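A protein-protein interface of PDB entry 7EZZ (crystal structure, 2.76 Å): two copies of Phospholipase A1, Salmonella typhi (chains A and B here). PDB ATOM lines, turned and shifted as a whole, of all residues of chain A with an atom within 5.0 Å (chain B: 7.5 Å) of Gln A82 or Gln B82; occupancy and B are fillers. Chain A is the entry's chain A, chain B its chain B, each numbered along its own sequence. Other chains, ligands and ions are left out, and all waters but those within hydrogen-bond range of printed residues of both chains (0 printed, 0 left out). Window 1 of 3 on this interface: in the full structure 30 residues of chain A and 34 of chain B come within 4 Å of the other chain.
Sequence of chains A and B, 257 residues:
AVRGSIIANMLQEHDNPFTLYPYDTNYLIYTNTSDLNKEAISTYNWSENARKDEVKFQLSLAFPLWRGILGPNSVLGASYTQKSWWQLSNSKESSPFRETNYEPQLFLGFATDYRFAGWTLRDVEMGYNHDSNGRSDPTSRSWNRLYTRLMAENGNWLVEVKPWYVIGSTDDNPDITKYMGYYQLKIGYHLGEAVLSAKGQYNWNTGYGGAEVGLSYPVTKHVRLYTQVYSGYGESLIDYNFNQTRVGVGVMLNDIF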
ATOM      1  N   PHE A  57      15.369  16.912  -0.823  1.00  0.00           N
ATOM      2  CA  PHE A  57      16.541  17.760  -0.920  1.00  0.00           C
ATOM      3  C   PHE A  57      17.538  17.197  -1.915  1.00  0.00           C
ATOM      4  O   PHE A  57      17.601  15.986  -2.125  1.00  0.00           O
ATOM      5  CB  PHE A  57      17.206  17.997   0.436  1.00  0.00           C
ATOM      6  CG  PHE A  57      17.753  16.780   1.137  1.00  0.00           C
ATOM      7  CD1 PHE A  57      16.922  15.973   1.891  1.00  0.00           C
ATOM      8  CD2 PHE A  57      19.105  16.482   1.109  1.00  0.00           C
ATOM      9  CE1 PHE A  57      17.417  14.888   2.599  1.00  0.00           C
ATOM     10  CE2 PHE A  57      19.599  15.377   1.786  1.00  0.00           C
ATOM     11  CZ  PHE A  57      18.759  14.580   2.530  1.00  0.00           C
ATOM     12  N   GLN A  58      18.326  18.120  -2.475  1.00  0.00           N
ATOM     13  CA  GLN A  58      19.372  17.810  -3.423  1.00  0.00           C
ATOM     14  C   GLN A  58      20.664  18.499  -2.978  1.00  0.00           C
ATOM     15  O   GLN A  58      20.661  19.662  -2.589  1.00  0.00           O
ATOM     16  CB  GLN A  58      18.925  18.285  -4.802  1.00  0.00           C
ATOM     17  CG  GLN A  58      19.909  17.909  -5.899  1.00  0.00           C
ATOM     18  CD  GLN A  58      19.310  18.241  -7.237  1.00  0.00           C
ATOM     19  OE1 GLN A  58      18.483  17.472  -7.742  1.00  0.00           O
ATOM     20  NE2 GLN A  58      19.686  19.399  -7.774  1.00  0.00           N
ATOM     21  N   LEU A  59      21.759  17.749  -3.006  1.00  0.00           N
ATOM     22  CA  LEU A  59      23.103  18.262  -2.852  1.00  0.00           C
ATOM     23  C   LEU A  59      23.783  18.014  -4.186  1.00  0.00           C
ATOM     24  O   LEU A  59      23.634  16.939  -4.752  1.00  0.00           O
ATOM     25  CB  LEU A  59      23.827  17.422  -1.800  1.00  0.00           C
ATOM     26  CG  LEU A  59      23.396  17.654  -0.349  1.00  0.00           C
ATOM     27  CD1 LEU A  59      23.496  16.358   0.462  1.00  0.00           C
ATOM     28  CD2 LEU A  59      24.229  18.755   0.307  1.00  0.00           C
ATOM     29  N   TYR A  80      29.066  15.054  -8.058  1.00  0.00           N
ATOM     30  CA  TYR A  80      28.223  14.159  -7.269  1.00  0.00           C
ATOM     31  C   TYR A  80      26.912  14.868  -6.968  1.00  0.00           C
ATOM     32  O   TYR A  80      26.920  15.955  -6.401  1.00  0.00           O
ATOM     33  CB  TYR A  80      28.886  13.720  -5.962  1.00  0.00           C
ATOM     34  CG  TYR A  80      27.967  12.922  -5.057  1.00  0.00           C
ATOM     35  CD1 TYR A  80      27.529  11.643  -5.412  1.00  0.00           C
ATOM     36  CD2 TYR A  80      27.520  13.431  -3.835  1.00  0.00           C
ATOM     37  CE1 TYR A  80      26.705  10.888  -4.590  1.00  0.00           C
ATOM     38  CE2 TYR A  80      26.671  12.692  -3.008  1.00  0.00           C
ATOM     39  CZ  TYR A  80      26.263  11.418  -3.390  1.00  0.00           C
ATOM     40  OH  TYR A  80      25.441  10.660  -2.605  1.00  0.00           O
ATOM     41  N   THR A  81      25.803  14.255  -7.406  1.00  0.00           N
ATOM     42  CA  THR A  81      24.483  14.790  -7.134  1.00  0.00           C
ATOM     43  C   THR A  81      23.703  13.752  -6.355  1.00  0.00           C
ATOM     44  O   THR A  81      23.681  12.594  -6.745  1.00  0.00           O
ATOM     45  CB  THR A  81      23.743  15.202  -8.408  1.00  0.00           C
ATOM     46  OG1 THR A  81      24.473  16.251  -9.049  1.00  0.00           O
ATOM     47  CG2 THR A  81      22.327  15.663  -8.127  1.00  0.00           C
ATOM     48  N   GLN A  82      23.050  14.203  -5.282  1.00  0.00           N
ATOM     49  CA  GLN A  82      22.274  13.333  -4.419  1.00  0.00           C
ATOM     50  C   GLN A  82      20.891  13.929  -4.207  1.00  0.00           C
ATOM     51  O   GLN A  82      20.769  15.093  -3.864  1.00  0.00           O
ATOM     52  CB  GLN A  82      22.945  13.142  -3.054  1.00  0.00           C
ATOM     53  CG  GLN A  82      22.197  12.129  -2.188  1.00  0.00           C
ATOM     54  CD  GLN A  82      22.714  11.967  -0.788  1.00  0.00           C
ATOM     55  OE1 GLN A  82      23.880  11.643  -0.553  1.00  0.00           O
ATOM     56  NE2 GLN A  82      21.805  12.153   0.153  1.00  0.00           N
ATOM     57  N   LYS A  83      19.858  13.102  -4.388  1.00  0.00           N
ATOM     58  CA  LYS A  83      18.476  13.524  -4.205  1.00  0.00           C
ATOM     59  C   LYS A  83      17.848  12.564  -3.207  1.00  0.00           C
ATOM     60  O   LYS A  83      18.044  11.361  -3.373  1.00  0.00           O
ATOM     61  CB  LYS A  83      17.686  13.424  -5.518  1.00  0.00           C
ATOM     62  CG  LYS A  83      17.848  14.554  -6.517  1.00  0.00           C
ATOM     63  CD  LYS A  83      17.395  14.121  -7.913  1.00  0.00           C
ATOM     64  N   SER A  84      17.124  13.087  -2.202  1.00  0.00           N
ATOM     65  CA  SER A  84      16.546  12.246  -1.150  1.00  0.00           C
ATOM     66  C   SER A  84      15.088  12.611  -0.890  1.00  0.00           C
ATOM     67  O   SER A  84      14.729  13.789  -0.902  1.00  0.00           O
ATOM     68  CB  SER A  84      17.322  12.310   0.157  1.00  0.00           C
ATOM     69  OG  SER A  84      18.733  12.100   0.009  1.00  0.00           O
ATOM     70  N   THR A 100      16.684   7.507  -2.115  1.00  0.00           N
ATOM     71  CA  THR A 100      17.772   8.408  -2.402  1.00  0.00           C
ATOM     72  C   THR A 100      18.341   7.992  -3.747  1.00  0.00           C
ATOM     73  O   THR A 100      18.435   6.801  -4.051  1.00  0.00           O
ATOM     74  CB  THR A 100      18.852   8.348  -1.312  1.00  0.00           C
ATOM     75  OG1 THR A 100      18.285   8.823  -0.086  1.00  0.00           O
ATOM     76  CG2 THR A 100      20.046   9.229  -1.603  1.00  0.00           C
ATOM     77  N   ASN A 101      18.683   8.997  -4.566  1.00  0.00           N
ATOM     78  CA  ASN A 101      19.399   8.750  -5.810  1.00  0.00           C
ATOM     79  C   ASN A 101      20.818   9.310  -5.686  1.00  0.00           C
ATOM     80  O   ASN A 101      21.011  10.459  -5.287  1.00  0.00           O
ATOM     81  CB  ASN A 101      18.624   9.252  -7.033  1.00  0.00           C
ATOM     82  CG  ASN A 101      17.308   8.540  -7.289  1.00  0.00           C
ATOM     83  OD1 ASN A 101      16.488   8.995  -8.081  1.00  0.00           O
ATOM     84  ND2 ASN A 101      17.085   7.413  -6.644  1.00  0.00           N
ATOM     85  N   TYR A 102      21.812   8.474  -6.008  1.00  0.00           N
ATOM     86  CA  TYR A 102      23.215   8.856  -5.945  1.00  0.00           C
ATOM     87  C   TYR A 102      23.772   8.944  -7.371  1.00  0.00           C
ATOM     88  O   TYR A 102      23.788   7.953  -8.112  1.00  0.00           O
ATOM     89  CB  TYR A 102      23.969   7.803  -5.130  1.00  0.00           C
ATOM     90  CG  TYR A 102      23.333   7.409  -3.815  1.00  0.00           C
ATOM     91  CD1 TYR A 102      23.616   8.089  -2.633  1.00  0.00           C
ATOM     92  CD2 TYR A 102      22.480   6.310  -3.738  1.00  0.00           C
ATOM     93  CE1 TYR A 102      23.082   7.686  -1.416  1.00  0.00           C
ATOM     94  CE2 TYR A 102      21.916   5.906  -2.540  1.00  0.00           C
ATOM     95  CZ  TYR A 102      22.223   6.597  -1.378  1.00  0.00           C
ATOM     96  OH  TYR A 102      21.641   6.195  -0.215  1.00  0.00           O
ATOM     97  N   GLU A 103      24.231  10.138  -7.769  1.00  0.00           N
ATOM     98  CA  GLU A 103      24.614  10.366  -9.156  1.00  0.00           C
ATOM     99  C   GLU A 103      26.048  10.898  -9.281  1.00  0.00           C
ATOM    100  O   GLU A 103      26.279  12.105  -9.440  1.00  0.00           O
ATOM    101  CB  GLU A 103      23.634  11.302  -9.859  1.00  0.00           C
ATOM    102  CG  GLU A 103      23.697  11.181 -11.378  1.00  0.00           C
ATOM    103  CD  GLU A 103      22.603  11.965 -12.073  1.00  0.00           C
ATOM    104  OE1 GLU A 103      21.465  11.902 -11.570  1.00  0.00           O
ATOM    105  OE2 GLU A 103      22.877  12.616 -13.109  1.00  0.00           O
ATOM    106  N   ASP B  24      32.959  20.199   7.937  1.00  0.00           N
ATOM    107  CA  ASP B  24      33.879  19.106   8.306  1.00  0.00           C
ATOM    108  C   ASP B  24      34.660  18.705   7.062  1.00  0.00           C
ATOM    109  O   ASP B  24      34.658  19.420   6.085  1.00  0.00           O
ATOM    110  CB  ASP B  24      33.105  17.915   8.852  1.00  0.00           C
ATOM    111  CG  ASP B  24      33.821  17.176   9.950  1.00  0.00           C
ATOM    112  OD1 ASP B  24      35.014  17.347  10.044  1.00  0.00           O
ATOM    113  OD2 ASP B  24      33.181  16.419  10.655  1.00  0.00           O
ATOM    114  N   THR B  25      35.342  17.588   7.136  1.00  0.00           N
ATOM    115  CA  THR B  25      36.105  17.126   5.988  1.00  0.00           C
ATOM    116  C   THR B  25      35.202  16.468   4.940  1.00  0.00           C
ATOM    117  O   THR B  25      34.143  15.940   5.259  1.00  0.00           O
ATOM    118  CB  THR B  25      37.251  16.180   6.377  1.00  0.00           C
ATOM    119  OG1 THR B  25      36.767  14.971   6.959  1.00  0.00           O
ATOM    120  CG2 THR B  25      38.288  16.817   7.265  1.00  0.00           C
ATOM    121  N   ASN B  26      35.633  16.533   3.674  1.00  0.00           N
ATOM    122  CA  ASN B  26      34.941  15.910   2.556  1.00  0.00           C
ATOM    123  C   ASN B  26      35.863  14.886   1.891  1.00  0.00           C
ATOM    124  O   ASN B  26      36.886  15.235   1.307  1.00  0.00           O
ATOM    125  CB  ASN B  26      34.476  16.959   1.545  1.00  0.00           C
ATOM    126  CG  ASN B  26      33.379  17.845   2.091  1.00  0.00           C
ATOM    127  OD1 ASN B  26      32.198  17.566   1.875  1.00  0.00           O
ATOM    128  ND2 ASN B  26      33.760  18.908   2.796  1.00  0.00           N
ATOM    129  N   TYR B  27      35.466  13.615   1.940  1.00  0.00           N
ATOM    130  CA  TYR B  27      36.327  12.570   1.437  1.00  0.00           C
ATOM    131  C   TYR B  27      35.541  11.355   0.950  1.00  0.00           C
ATOM    132  O   TYR B  27      34.375  11.157   1.316  1.00  0.00           O
ATOM    133  CB  TYR B  27      37.312  12.144   2.523  1.00  0.00           C
ATOM    134  CG  TYR B  27      36.735  11.515   3.773  1.00  0.00           C
ATOM    135  CD1 TYR B  27      36.381  10.167   3.816  1.00  0.00           C
ATOM    136  CD2 TYR B  27      36.595  12.258   4.941  1.00  0.00           C
ATOM    137  CE1 TYR B  27      35.890   9.583   4.979  1.00  0.00           C
ATOM    138  CE2 TYR B  27      36.108  11.690   6.107  1.00  0.00           C
ATOM    139  CZ  TYR B  27      35.768  10.345   6.132  1.00  0.00           C
ATOM    140  OH  TYR B  27      35.266   9.771   7.268  1.00  0.00           O
ATOM    141  N   PHE B  57      32.174   7.455   2.571  1.00  0.00           N
ATOM    142  CA  PHE B  57      32.375   8.849   2.215  1.00  0.00           C
ATOM    143  C   PHE B  57      31.626   9.763   3.165  1.00  0.00           C
ATOM    144  O   PHE B  57      30.605   9.384   3.741  1.00  0.00           O
ATOM    145  CB  PHE B  57      32.003   9.135   0.765  1.00  0.00           C
ATOM    146  CG  PHE B  57      30.560   8.906   0.390  1.00  0.00           C
ATOM    147  CD1 PHE B  57      30.090   7.632   0.093  1.00  0.00           C
ATOM    148  CD2 PHE B  57      29.678   9.972   0.272  1.00  0.00           C
ATOM    149  CE1 PHE B  57      28.772   7.421  -0.292  1.00  0.00           C
ATOM    150  CE2 PHE B  57      28.361   9.759  -0.127  1.00  0.00           C
ATOM    151  CZ  PHE B  57      27.905   8.480  -0.405  1.00  0.00           C
ATOM    152  N   GLN B  58      32.164  10.973   3.280  1.00  0.00           N
ATOM    153  CA  GLN B  58      31.591  12.023   4.096  1.00  0.00           C
ATOM    154  C   GLN B  58      31.491  13.288   3.251  1.00  0.00           C
ATOM    155  O   GLN B  58      32.412  13.650   2.532  1.00  0.00           O
ATOM    156  CB  GLN B  58      32.501  12.238   5.306  1.00  0.00           C
ATOM    157  CG  GLN B  58      31.841  13.012   6.438  1.00  0.00           C
ATOM    158  CD  GLN B  58      32.808  13.419   7.510  1.00  0.00           C
ATOM    159  OE1 GLN B  58      32.907  12.770   8.534  1.00  0.00           O
ATOM    160  NE2 GLN B  58      33.557  14.478   7.275  1.00  0.00           N
ATOM    161  N   LEU B  59      30.324  13.919   3.295  1.00  0.00           N
ATOM    162  CA  LEU B  59      30.082  15.250   2.757  1.00  0.00           C
ATOM    163  C   LEU B  59      29.858  16.148   3.957  1.00  0.00           C
ATOM    164  O   LEU B  59      29.179  15.737   4.890  1.00  0.00           O
ATOM    165  CB  LEU B  59      28.766  15.210   1.986  1.00  0.00           C
ATOM    166  CG  LEU B  59      28.708  14.266   0.798  1.00  0.00           C
ATOM    167  CD1 LEU B  59      27.353  13.546   0.752  1.00  0.00           C
ATOM    168  CD2 LEU B  59      28.977  15.050  -0.486  1.00  0.00           C
ATOM    169  N   SER B  60      30.381  17.369   3.911  1.00  0.00           N
ATOM    170  CA  SER B  60      30.110  18.293   4.993  1.00  0.00           C
ATOM    171  C   SER B  60      30.198  19.742   4.529  1.00  0.00           C
ATOM    172  O   SER B  60      31.240  20.154   4.038  1.00  0.00           O
ATOM    173  CB  SER B  60      31.005  18.011   6.153  1.00  0.00           C
ATOM    174  OG  SER B  60      30.699  18.885   7.223  1.00  0.00           O
ATOM    175  N   LEU B  61      29.081  20.488   4.717  1.00  0.00           N
ATOM    176  CA  LEU B  61      28.905  21.860   4.241  1.00  0.00           C
ATOM    177  C   LEU B  61      28.463  22.768   5.373  1.00  0.00           C
ATOM    178  O   LEU B  61      27.671  22.341   6.209  1.00  0.00           O
ATOM    179  CB  LEU B  61      27.800  21.926   3.188  1.00  0.00           C
ATOM    180  CG  LEU B  61      28.053  21.260   1.836  1.00  0.00           C
ATOM    181  CD1 LEU B  61      26.910  21.590   0.877  1.00  0.00           C
ATOM    182  CD2 LEU B  61      29.369  21.733   1.237  1.00  0.00           C
ATOM    183  N   TYR B  80      25.558  20.675   7.448  1.00  0.00           N
ATOM    184  CA  TYR B  80      25.047  19.345   7.157  1.00  0.00           C
ATOM    185  C   TYR B  80      26.227  18.400   6.920  1.00  0.00           C
ATOM    186  O   TYR B  80      27.045  18.634   6.026  1.00  0.00           O
ATOM    187  CB  TYR B  80      24.132  19.374   5.928  1.00  0.00           C
ATOM    188  CG  TYR B  80      23.687  17.997   5.492  1.00  0.00           C
ATOM    189  CD1 TYR B  80      22.827  17.257   6.298  1.00  0.00           C
ATOM    190  CD2 TYR B  80      24.139  17.409   4.313  1.00  0.00           C
ATOM    191  CE1 TYR B  80      22.418  15.975   5.949  1.00  0.00           C
ATOM    192  CE2 TYR B  80      23.722  16.138   3.941  1.00  0.00           C
ATOM    193  CZ  TYR B  80      22.856  15.414   4.761  1.00  0.00           C
ATOM    194  OH  TYR B  80      22.433  14.141   4.478  1.00  0.00           O
ATOM    195  N   THR B  81      26.298  17.347   7.735  1.00  0.00           N
ATOM    196  CA  THR B  81      27.327  16.343   7.551  1.00  0.00           C
ATOM    197  C   THR B  81      26.639  15.011   7.291  1.00  0.00           C
ATOM    198  O   THR B  81      25.680  14.660   7.969  1.00  0.00           O
ATOM    199  CB  THR B  81      28.283  16.251   8.749  1.00  0.00           C
ATOM    200  OG1 THR B  81      28.964  17.501   8.876  1.00  0.00           O
ATOM    201  CG2 THR B  81      29.284  15.128   8.621  1.00  0.00           C
ATOM    202  N   GLN B  82      27.150  14.295   6.293  1.00  0.00           N
ATOM    203  CA  GLN B  82      26.578  13.020   5.902  1.00  0.00           C
ATOM    204  C   GLN B  82      27.691  12.000   5.746  1.00  0.00           C
ATOM    205  O   GLN B  82      28.669  12.257   5.065  1.00  0.00           O
ATOM    206  CB  GLN B  82      25.828  13.125   4.575  1.00  0.00           C
ATOM    207  CG  GLN B  82      25.001  11.888   4.280  1.00  0.00           C
ATOM    208  CD  GLN B  82      24.563  11.801   2.844  1.00  0.00           C
ATOM    209  OE1 GLN B  82      23.762  12.601   2.378  1.00  0.00           O
ATOM    210  NE2 GLN B  82      25.083  10.809   2.136  1.00  0.00           N
ATOM    211  N   LYS B  83      27.530  10.833   6.376  1.00  0.00           N
ATOM    212  CA  LYS B  83      28.486   9.740   6.266  1.00  0.00           C
ATOM    213  C   LYS B  83      27.734   8.528   5.740  1.00  0.00           C
ATOM    214  O   LYS B  83      26.639   8.260   6.232  1.00  0.00           O
ATOM    215  CB  LYS B  83      29.120   9.378   7.609  1.00  0.00           C
ATOM    216  CG  LYS B  83      29.574  10.536   8.490  1.00  0.00           C
ATOM    217  CD  LYS B  83      30.626  10.191   9.506  1.00  0.00           C
ATOM    218  CE  LYS B  83      30.211  10.627  10.894  1.00  0.00           C
ATOM    219  NZ  LYS B  83      30.572  12.047  11.113  1.00  0.00           N
ATOM    220  N   SER B  84      28.320   7.835   4.744  1.00  0.00           N
ATOM    221  CA  SER B  84      27.681   6.680   4.132  1.00  0.00           C
ATOM    222  C   SER B  84      28.641   5.497   4.048  1.00  0.00           C
ATOM    223  O   SER B  84      29.816   5.659   3.760  1.00  0.00           O
ATOM    224  CB  SER B  84      27.166   7.007   2.756  1.00  0.00           C
ATOM    225  OG  SER B  84      26.043   7.873   2.767  1.00  0.00           O
ATOM    226  N   TRP B  85      28.104   4.293   4.249  1.00  0.00           N
ATOM    227  CA  TRP B  85      28.841   3.050   4.104  1.00  0.00           C
ATOM    228  C   TRP B  85      28.133   2.205   3.057  1.00  0.00           C
ATOM    229  O   TRP B  85      26.968   1.846   3.217  1.00  0.00           O
ATOM    230  CB  TRP B  85      28.908   2.304   5.443  1.00  0.00           C
ATOM    231  CG  TRP B  85      29.779   2.974   6.461  1.00  0.00           C
ATOM    232  CD1 TRP B  85      31.077   2.673   6.771  1.00  0.00           C
ATOM    233  CD2 TRP B  85      29.412   4.083   7.303  1.00  0.00           C
ATOM    234  NE1 TRP B  85      31.552   3.519   7.735  1.00  0.00           N
ATOM    235  CE2 TRP B  85      30.554   4.398   8.083  1.00  0.00           C
ATOM    236  CE3 TRP B  85      28.258   4.869   7.446  1.00  0.00           C
ATOM    237  CZ2 TRP B  85      30.555   5.443   9.013  1.00  0.00           C
ATOM    238  CZ3 TRP B  85      28.261   5.898   8.365  1.00  0.00           C
ATOM    239  CH2 TRP B  85      29.395   6.177   9.137  1.00  0.00           C
ATOM    240  N   PHE B  97      23.468   0.263   0.067  1.00  0.00           N
ATOM    241  CA  PHE B  97      24.021   1.033   1.168  1.00  0.00           C
ATOM    242  C   PHE B  97      23.703   0.307   2.464  1.00  0.00           C
ATOM    243  O   PHE B  97      22.565  -0.084   2.688  1.00  0.00           O
ATOM    244  CB  PHE B  97      23.418   2.436   1.207  1.00  0.00           C
ATOM    245  CG  PHE B  97      24.162   3.451   0.381  1.00  0.00           C
ATOM    246  CD1 PHE B  97      24.337   3.270  -0.989  1.00  0.00           C
ATOM    247  CD2 PHE B  97      24.725   4.582   0.972  1.00  0.00           C
ATOM    248  CE1 PHE B  97      25.043   4.200  -1.751  1.00  0.00           C
ATOM    249  CE2 PHE B  97      25.432   5.508   0.204  1.00  0.00           C
ATOM    250  CZ  PHE B  97      25.583   5.327  -1.152  1.00  0.00           C
ATOM    251  N   GLU B  99      24.394   1.769   5.537  1.00  0.00           N
ATOM    252  CA  GLU B  99      24.146   2.747   6.589  1.00  0.00           C
ATOM    253  C   GLU B  99      24.532   4.145   6.110  1.00  0.00           C
ATOM    254  O   GLU B  99      25.552   4.310   5.459  1.00  0.00           O
ATOM    255  CB  GLU B  99      24.936   2.401   7.857  1.00  0.00           C
ATOM    256  CG  GLU B  99      24.986   3.513   8.899  1.00  0.00           C
ATOM    257  CD  GLU B  99      23.783   3.557   9.834  1.00  0.00           C
ATOM    258  OE1 GLU B  99      22.712   2.992   9.450  1.00  0.00           O
ATOM    259  OE2 GLU B  99      23.899   4.153  10.940  1.00  0.00           O
ATOM    260  N   THR B 100      23.707   5.141   6.450  1.00  0.00           N
ATOM    261  CA  THR B 100      24.023   6.542   6.261  1.00  0.00           C
ATOM    262  C   THR B 100      23.691   7.261   7.563  1.00  0.00           C
ATOM    263  O   THR B 100      22.702   6.944   8.207  1.00  0.00           O
ATOM    264  CB  THR B 100      23.204   7.167   5.118  1.00  0.00           C
ATOM    265  OG1 THR B 100      23.406   6.442   3.898  1.00  0.00           O
ATOM    266  CG2 THR B 100      23.544   8.625   4.877  1.00  0.00           C
ATOM    267  N   ASN B 101      24.527   8.224   7.952  1.00  0.00           N
ATOM    268  CA  ASN B 101      24.234   9.089   9.081  1.00  0.00           C
ATOM    269  C   ASN B 101      24.024  10.513   8.553  1.00  0.00           C
ATOM    270  O   ASN B 101      24.863  11.039   7.830  1.00  0.00           O
ATOM    271  CB  ASN B 101      25.274   8.983  10.212  1.00  0.00           C
ATOM    272  CG  ASN B 101      25.362   7.612  10.862  1.00  0.00           C
ATOM    273  OD1 ASN B 101      26.305   7.305  11.581  1.00  0.00           O
ATOM    274  ND2 ASN B 101      24.370   6.766  10.638  1.00  0.00           N
ATOM    275  N   TYR B 102      22.894  11.131   8.928  1.00  0.00           N
ATOM    276  CA  TYR B 102      22.554  12.478   8.523  1.00  0.00           C
ATOM    277  C   TYR B 102      22.668  13.413   9.722  1.00  0.00           C
ATOM    278  O   TYR B 102      21.955  13.248  10.704  1.00  0.00           O
ATOM    279  CB  TYR B 102      21.132  12.481   7.968  1.00  0.00           C
ATOM    280  CG  TYR B 102      20.826  11.390   6.969  1.00  0.00           C
ATOM    281  CD1 TYR B 102      20.507  10.092   7.365  1.00  0.00           C
ATOM    282  CD2 TYR B 102      20.784  11.677   5.617  1.00  0.00           C
ATOM    283  CE1 TYR B 102      20.198   9.101   6.446  1.00  0.00           C
ATOM    284  CE2 TYR B 102      20.469  10.702   4.683  1.00  0.00           C
ATOM    285  CZ  TYR B 102      20.180   9.415   5.095  1.00  0.00           C
ATOM    286  OH  TYR B 102      19.925   8.470   4.145  1.00  0.00           O
ATOM    287  N   GLU B 103      23.544  14.426   9.633  1.00  0.00           N
ATOM    288  CA  GLU B 103      23.865  15.247  10.802  1.00  0.00           C
ATOM    289  C   GLU B 103      23.688  16.743  10.518  1.00  0.00           C
ATOM    290  O   GLU B 103      24.657  17.473  10.258  1.00  0.00           O
ATOM    291  CB  GLU B 103      25.282  14.978  11.299  1.00  0.00           C
ATOM    292  CG  GLU B 103      25.469  15.314  12.758  1.00  0.00           C
ATOM    293  CD  GLU B 103      26.817  14.888  13.321  1.00  0.00           C
ATOM    294  OE1 GLU B 103      27.261  13.790  12.955  1.00  0.00           O
ATOM    295  OE2 GLU B 103      27.409  15.628  14.146  1.00  0.00           O
ATOM    296  N   PRO B 104      22.433  17.257  10.534  1.00  0.00           N
ATOM    297  CA  PRO B 104      22.192  18.694  10.407  1.00  0.00           C
ATOM    298  C   PRO B 104      22.400  19.428  11.727  1.00  0.00           C
ATOM    299  O   PRO B 104      22.149  18.882  12.797  1.00  0.00           O
ATOM    300  CB  PRO B 104      20.720  18.732   9.977  1.00  0.00           C
ATOM    301  CG  PRO B 104      20.100  17.543  10.670  1.00  0.00           C
ATOM    302  CD  PRO B 104      21.180  16.477  10.601  1.00  0.00           C
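The side-chain amide nitrogen (NE2) of Gln A82 lies within hydrogen-bond range of the side-chain amide oxygen (OE1) of Gln B82, 3.0 Å away.
Leu B61 touches Leu A59. Leu A59 touches Tyr B80 (CD1 to CE2, 3.5 Å). Tyr A80 touches Phe B57 (OH to CE2, 3.9 Å). Leu B59 touches Tyr A80. Phe B97 touches Tyr A102 (CZ to CE1, 3.4 Å).
Of the printed residues of chain B, Leu A59 touches Leu B61 (3.9 Å) and Tyr B80 (3.5 Å). Gln A82 touches just one residue of chain B: Gln B82 (3.0 Å). Of the printed residues of chain A, Leu B59 touches Tyr A80 (3.9 Å). Of the printed residues of chain A, Leu B61 touches Leu A59. Gln B82 touches just one residue of chain A: Gln A82. The nearest printed residue of chain A that does not touch Leu B59 is Gln A82 (4.2 Å).
O of Phe B57 is in hydrogen-bond range of N of Ser B84 (2.9 Å). O of Leu A59 is in hydrogen-bond range of N of Gln A82 (2.8 Å). NE2 of Gln B82 sits at hydrogen-bond distance from OG of Ser B84, at 3.2 Å. O of Leu B59 lies within hydrogen-bond range of N of Gln B82, 2.9 Å away. O of Leu B61 is in hydrogen-bond range of N of Tyr B80. The side-chain hydroxyl (OG) of Ser A84 is in hydrogen-bond range of the side-chain amide nitrogen (NE2) of Gln A82 (3.1 Å).
Leu A59 touches Tyr B80, and with the chains exchanged Tyr A80 touches Leu B59. Tyr A80 touches Phe B57, but with the chains exchanged Phe A57 does not touch Tyr B80 (4.1 Å). Gln A82 touches its own counterpart, Gln B82.
Of the 12 printed residues of chain A, 4 touch a printed residue of chain B. Hydrophobic or aromatic side chains of chain A within 4 Å of the printed part of chain B: Leu A59, Tyr A80 and Tyr A102.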
